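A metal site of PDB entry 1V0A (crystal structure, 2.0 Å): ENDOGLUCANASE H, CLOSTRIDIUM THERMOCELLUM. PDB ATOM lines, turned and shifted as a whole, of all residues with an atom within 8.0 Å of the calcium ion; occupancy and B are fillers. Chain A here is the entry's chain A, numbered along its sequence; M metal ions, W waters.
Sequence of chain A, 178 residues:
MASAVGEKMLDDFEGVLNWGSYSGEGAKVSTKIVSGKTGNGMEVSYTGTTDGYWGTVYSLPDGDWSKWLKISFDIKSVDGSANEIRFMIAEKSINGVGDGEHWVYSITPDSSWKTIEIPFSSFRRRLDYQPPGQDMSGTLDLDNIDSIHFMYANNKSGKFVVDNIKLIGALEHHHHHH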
ATOM      1  N   MET A   9       9.022  22.143 -13.725  1.00  0.00           N
ATOM      2  CA  MET A   9       8.360  20.859 -13.572  1.00  0.00           C
ATOM      3  C   MET A   9       7.540  20.811 -12.289  1.00  0.00           C
ATOM      4  O   MET A   9       8.017  21.201 -11.223  1.00  0.00           O
ATOM      5  CB  MET A   9       9.386  19.717 -13.595  1.00  0.00           C
ATOM      6  CG  MET A   9       8.800  18.303 -13.642  1.00  0.00           C
ATOM      7  SD  MET A   9       7.843  17.856 -15.308  1.00  0.00           S
ATOM      8  CE  MET A   9       9.370  17.671 -16.513  1.00  0.00           C
ATOM      9  N   ASP A  11       5.339  17.808 -11.814  1.00  0.00           N
ATOM     10  CA  ASP A  11       5.364  16.366 -11.546  1.00  0.00           C
ATOM     11  C   ASP A  11       5.757  15.544 -12.768  1.00  0.00           C
ATOM     12  O   ASP A  11       5.038  15.507 -13.767  1.00  0.00           O
ATOM     13  CB  ASP A  11       4.002  15.883 -11.010  1.00  0.00           C
ATOM     14  CG  ASP A  11       4.147  14.819  -9.932  1.00  0.00           C
ATOM     15  OD1 ASP A  11       5.138  14.055  -9.965  1.00  0.00           O
ATOM     16  OD2 ASP A  11       3.311  14.674  -9.012  1.00  0.00           O
ATOM     17  N   ASP A  12       6.909  14.883 -12.667  1.00  0.00           N
ATOM     18  CA  ASP A  12       7.317  13.889 -13.669  1.00  0.00           C
ATOM     19  C   ASP A  12       7.092  12.470 -13.136  1.00  0.00           C
ATOM     20  O   ASP A  12       7.418  11.479 -13.801  1.00  0.00           O
ATOM     21  CB  ASP A  12       8.767  14.100 -14.121  1.00  0.00           C
ATOM     22  CG  ASP A  12       9.767  14.107 -12.961  1.00  0.00           C
ATOM     23  OD1 ASP A  12       9.422  13.704 -11.837  1.00  0.00           O
ATOM     24  OD2 ASP A  12      10.946  14.496 -13.107  1.00  0.00           O
ATOM     25  N   PHE A  13       6.526  12.405 -11.926  1.00  0.00           N
ATOM     26  CA  PHE A  13       6.151  11.158 -11.249  1.00  0.00           C
ATOM     27  C   PHE A  13       7.328  10.242 -10.871  1.00  0.00           C
ATOM     28  O   PHE A  13       7.130   9.064 -10.554  1.00  0.00           O
ATOM     29  CB  PHE A  13       5.055  10.413 -12.021  1.00  0.00           C
ATOM     30  CG  PHE A  13       3.797  11.212 -12.189  1.00  0.00           C
ATOM     31  CD1 PHE A  13       3.553  11.912 -13.370  1.00  0.00           C
ATOM     32  CD2 PHE A  13       2.875  11.303 -11.145  1.00  0.00           C
ATOM     33  CE1 PHE A  13       2.396  12.664 -13.518  1.00  0.00           C
ATOM     34  CE2 PHE A  13       1.710  12.063 -11.288  1.00  0.00           C
ATOM     35  CZ  PHE A  13       1.474  12.734 -12.478  1.00  0.00           C
ATOM     36  N   GLU A  14       8.539  10.790 -10.888  1.00  0.00           N
ATOM     37  CA  GLU A  14       9.736  10.044 -10.498  1.00  0.00           C
ATOM     38  C   GLU A  14      10.085  10.264  -9.028  1.00  0.00           C
ATOM     39  O   GLU A  14      10.892   9.511  -8.456  1.00  0.00           O
ATOM     40  CB  GLU A  14      10.929  10.395 -11.396  1.00  0.00           C
ATOM     41  CG  GLU A  14      10.609  10.583 -12.878  1.00  0.00           C
ATOM     42  CD  GLU A  14      10.102   9.324 -13.569  1.00  0.00           C
ATOM     43  OE1 GLU A  14       9.662   9.438 -14.734  1.00  0.00           O
ATOM     44  OE2 GLU A  14      10.135   8.229 -12.975  1.00  0.00           O
ATOM     45  N   GLY A  15       9.486  11.284  -8.414  1.00  0.00           N
ATOM     46  CA  GLY A  15       9.718  11.593  -7.015  1.00  0.00           C
ATOM     47  C   GLY A  15       8.601  11.116  -6.112  1.00  0.00           C
ATOM     48  O   GLY A  15       8.068  10.019  -6.292  1.00  0.00           O
ATOM     49  N   VAL A  34       2.352   3.860 -12.899  1.00  0.00           N
ATOM     50  CA  VAL A  34       2.654   2.900 -13.955  1.00  0.00           C
ATOM     51  C   VAL A  34       3.774   3.456 -14.844  1.00  0.00           C
ATOM     52  O   VAL A  34       4.419   4.446 -14.492  1.00  0.00           O
ATOM     53  CB  VAL A  34       1.404   2.564 -14.818  1.00  0.00           C
ATOM     54  CG1 VAL A  34       0.374   1.777 -14.020  1.00  0.00           C
ATOM     55  CG2 VAL A  34       0.786   3.825 -15.429  1.00  0.00           C
ATOM     56  N   SER A  35       4.007   2.809 -15.985  1.00  0.00           N
ATOM     57  CA  SER A  35       4.939   3.341 -16.989  1.00  0.00           C
ATOM     58  C   SER A  35       4.343   4.581 -17.649  1.00  0.00           C
ATOM     59  O   SER A  35       3.202   4.556 -18.119  1.00  0.00           O
ATOM     60  CB  SER A  35       5.259   2.279 -18.041  1.00  0.00           C
ATOM     61  OG  SER A  35       5.795   1.105 -17.452  1.00  0.00           O
ATOM     62  N   GLY A  36       5.118   5.662 -17.661  1.00  0.00           N
ATOM     63  CA  GLY A  36       4.697   6.908 -18.281  1.00  0.00           C
ATOM     64  C   GLY A  36       5.327   7.120 -19.641  1.00  0.00           C
ATOM     65  O   GLY A  36       5.708   6.148 -20.308  1.00  0.00           O
ATOM     66  N   LYS A  37       5.416   8.382 -20.058  1.00  0.00           N
ATOM     67  CA  LYS A  37       6.091   8.745 -21.309  1.00  0.00           C
ATOM     68  C   LYS A  37       7.571   8.373 -21.189  1.00  0.00           C
ATOM     69  O   LYS A  37       8.115   7.672 -22.042  1.00  0.00           O
ATOM     70  CB  LYS A  37       5.920  10.236 -21.596  1.00  0.00           C
ATOM     71  CG  LYS A  37       6.668  10.754 -22.818  1.00  0.00           C
ATOM     72  CD  LYS A  37       5.802  10.728 -24.072  1.00  0.00           C
ATOM     73  CE  LYS A  37       6.584  11.204 -25.297  1.00  0.00           C
ATOM     74  N   THR A  38       8.204   8.847 -20.116  1.00  0.00           N
ATOM     75  CA  THR A  38       9.529   8.408 -19.705  1.00  0.00           C
ATOM     76  C   THR A  38       9.453   8.063 -18.228  1.00  0.00           C
ATOM     77  O   THR A  38       8.839   8.799 -17.447  1.00  0.00           O
ATOM     78  CB  THR A  38      10.587   9.502 -19.957  1.00  0.00           C
ATOM     79  OG1 THR A  38      10.079  10.778 -19.542  1.00  0.00           O
ATOM     80  CG2 THR A  38      10.853   9.689 -21.448  1.00  0.00           C
ATOM     81  N   GLY A  39      10.073   6.955 -17.849  1.00  0.00           N
ATOM     82  CA  GLY A  39      10.019   6.475 -16.477  1.00  0.00           C
ATOM     83  C   GLY A  39       8.598   6.211 -16.015  1.00  0.00           C
ATOM     84  O   GLY A  39       7.823   5.539 -16.694  1.00  0.00           O
ATOM     85  N   ASN A  40       8.254   6.768 -14.860  1.00  0.00           N
ATOM     86  CA  ASN A  40       6.930   6.588 -14.259  1.00  0.00           C
ATOM     87  C   ASN A  40       5.904   7.599 -14.751  1.00  0.00           C
ATOM     88  O   ASN A  40       6.248   8.718 -15.164  1.00  0.00           O
ATOM     89  CB  ASN A  40       7.013   6.655 -12.733  1.00  0.00           C
ATOM     90  CG  ASN A  40       7.773   5.489 -12.118  1.00  0.00           C
ATOM     91  OD1 ASN A  40       7.655   4.344 -12.571  1.00  0.00           O
ATOM     92  ND2 ASN A  40       8.546   5.770 -11.074  1.00  0.00           N
ATOM     93  N   GLY A  41       4.640   7.192 -14.713  1.00  0.00           N
ATOM     94  CA  GLY A  41       3.515   8.079 -14.941  1.00  0.00           C
ATOM     95  C   GLY A  41       2.374   7.664 -14.036  1.00  0.00           C
ATOM     96  O   GLY A  41       2.462   6.625 -13.368  1.00  0.00           O
ATOM     97  N   MET A  42       1.312   8.457 -13.986  1.00  0.00           N
ATOM     98  CA  MET A  42       0.147   8.119 -13.167  1.00  0.00           C
ATOM     99  C   MET A  42      -1.039   7.707 -14.020  1.00  0.00           C
ATOM    100  O   MET A  42      -1.514   8.478 -14.868  1.00  0.00           O
ATOM    101  CB  MET A  42      -0.228   9.277 -12.239  1.00  0.00           C
ATOM    102  CG  MET A  42      -1.471   9.018 -11.389  1.00  0.00           C
ATOM    103  SD  MET A  42      -2.061  10.545 -10.316  1.00  0.00           S
ATOM    104  CE  MET A  42      -2.483  11.803 -11.738  1.00  0.00           C
ATOM    105  N   ASP A  74       1.823  15.437 -20.713  1.00  0.00           N
ATOM    106  CA  ASP A  74       1.685  14.321 -21.660  1.00  0.00           C
ATOM    107  C   ASP A  74       0.514  13.459 -21.204  1.00  0.00           C
ATOM    108  O   ASP A  74       0.349  13.210 -20.015  1.00  0.00           O
ATOM    109  CB  ASP A  74       2.969  13.486 -21.694  1.00  0.00           C
ATOM    110  CG  ASP A  74       4.107  14.190 -22.393  1.00  0.00           C
ATOM    111  OD1 ASP A  74       5.174  14.382 -21.762  1.00  0.00           O
ATOM    112  OD2 ASP A  74       4.032  14.600 -23.578  1.00  0.00           O
ATOM    113  N   TRP A 113       0.709   8.739 -27.096  1.00  0.00           N
ATOM    114  CA  TRP A 113       1.178   9.844 -26.270  1.00  0.00           C
ATOM    115  C   TRP A 113       1.163  11.161 -27.033  1.00  0.00           C
ATOM    116  O   TRP A 113       1.716  11.257 -28.128  1.00  0.00           O
ATOM    117  CB  TRP A 113       2.608   9.577 -25.764  1.00  0.00           C
ATOM    118  CG  TRP A 113       2.681   8.650 -24.589  1.00  0.00           C
ATOM    119  CD1 TRP A 113       3.175   7.379 -24.577  1.00  0.00           C
ATOM    120  CD2 TRP A 113       2.277   8.931 -23.243  1.00  0.00           C
ATOM    121  NE1 TRP A 113       3.093   6.849 -23.315  1.00  0.00           N
ATOM    122  CE2 TRP A 113       2.544   7.775 -22.472  1.00  0.00           C
ATOM    123  CE3 TRP A 113       1.709  10.047 -22.602  1.00  0.00           C
ATOM    124  CZ2 TRP A 113       2.269   7.701 -21.101  1.00  0.00           C
ATOM    125  CZ3 TRP A 113       1.438   9.975 -21.245  1.00  0.00           C
ATOM    126  CH2 TRP A 113       1.714   8.804 -20.504  1.00  0.00           C
ATOM    127  N   VAL A 162      -1.010  10.007 -17.309  1.00  0.00           N
ATOM    128  CA  VAL A 162      -0.418  11.331 -17.443  1.00  0.00           C
ATOM    129  C   VAL A 162       1.053  11.334 -17.028  1.00  0.00           C
ATOM    130  O   VAL A 162       1.484  10.492 -16.231  1.00  0.00           O
ATOM    131  CB  VAL A 162      -1.193  12.425 -16.635  1.00  0.00           C
ATOM    132  CG1 VAL A 162      -2.594  12.620 -17.204  1.00  0.00           C
ATOM    133  CG2 VAL A 162      -1.246  12.089 -15.156  1.00  0.00           C
ATOM    134  N   ASP A 163       1.802  12.271 -17.589  1.00  0.00           N
ATOM    135  CA  ASP A 163       3.221  12.428 -17.288  1.00  0.00           C
ATOM    136  C   ASP A 163       3.653  13.873 -17.555  1.00  0.00           C
ATOM    137  O   ASP A 163       2.940  14.628 -18.208  1.00  0.00           O
ATOM    138  CB  ASP A 163       4.064  11.473 -18.147  1.00  0.00           C
ATOM    139  CG  ASP A 163       5.387  11.101 -17.483  1.00  0.00           C
ATOM    140  OD1 ASP A 163       5.751  11.693 -16.446  1.00  0.00           O
ATOM    141  OD2 ASP A 163       6.133  10.210 -17.941  1.00  0.00           O
ATOM    142  N   ASN A 164       4.828  14.232 -17.025  1.00  0.00           N
ATOM    143  CA  ASN A 164       5.486  15.512 -17.325  1.00  0.00           C
ATOM    144  C   ASN A 164       4.584  16.743 -17.198  1.00  0.00           C
ATOM    145  O   ASN A 164       4.479  17.556 -18.130  1.00  0.00           O
ATOM    146  CB  ASN A 164       6.168  15.459 -18.695  1.00  0.00           C
ATOM    147  CG  ASN A 164       7.159  14.315 -18.815  1.00  0.00           C
ATOM    148  OD1 ASN A 164       7.967  14.091 -17.911  1.00  0.00           O
ATOM    149  ND2 ASN A 164       7.094  13.580 -19.915  1.00  0.00           N
ATOM    150  N   ILE A 165       3.932  16.876 -16.053  1.00  0.00           N
ATOM    151  CA  ILE A 165       3.122  18.055 -15.767  1.00  0.00           C
ATOM    152  C   ILE A 165       4.046  19.200 -15.375  1.00  0.00           C
ATOM    153  O   ILE A 165       4.826  19.081 -14.425  1.00  0.00           O
ATOM    154  CB  ILE A 165       2.064  17.746 -14.679  1.00  0.00           C
ATOM    155  CG1 ILE A 165       1.158  16.603 -15.147  1.00  0.00           C
ATOM    156  CG2 ILE A 165       1.229  18.992 -14.367  1.00  0.00           C
ATOM    157  CD1 ILE A 165       0.548  15.806 -14.038  1.00  0.00           C
HETATM  158 CA    CA M   1       7.760  10.313 -15.917  1.00  0.00          CA
HETATM  159  O   HOH W   1       9.172  11.943 -16.964  1.00  0.00           O
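O of Asp 163 sits at hydrogen-bond distance from N of Asp 74 (2.9 Å).
The backbone NH (N) of Lys 37 lies close to the side-chain carboxylate (OD2) of Asp 163 (2.9 Å).
Of the 21 residues printed, 5 come within 4 Å of the calcium ion.
The nearest printed residue that does not touch the calcium ion is Gly 39 (4.2 Å).
O of Asn 40 is bound to the calcium ion, at 2.3 Å.
Water W1 binds the calcium ion.
OE1 of Glu 14 binds the calcium ion (2.4 Å).
The calcium ion is bound by the backbone carbonyl oxygen (O) of Thr 38, 2.4 Å away.
The calcium ion is bound by O of Asp 12 (2.4 Å).
The calcium ion is bound by OD1 of Asp 163, 2.5 Å away.
The calcium ion is bound by the side-chain carboxylate (OD2) of Asp 163 (2.6 Å).
Water W1 bridges OD1 of Asn 164 (2.6 Å) and OG1 of Thr 38 (3.0 Å).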
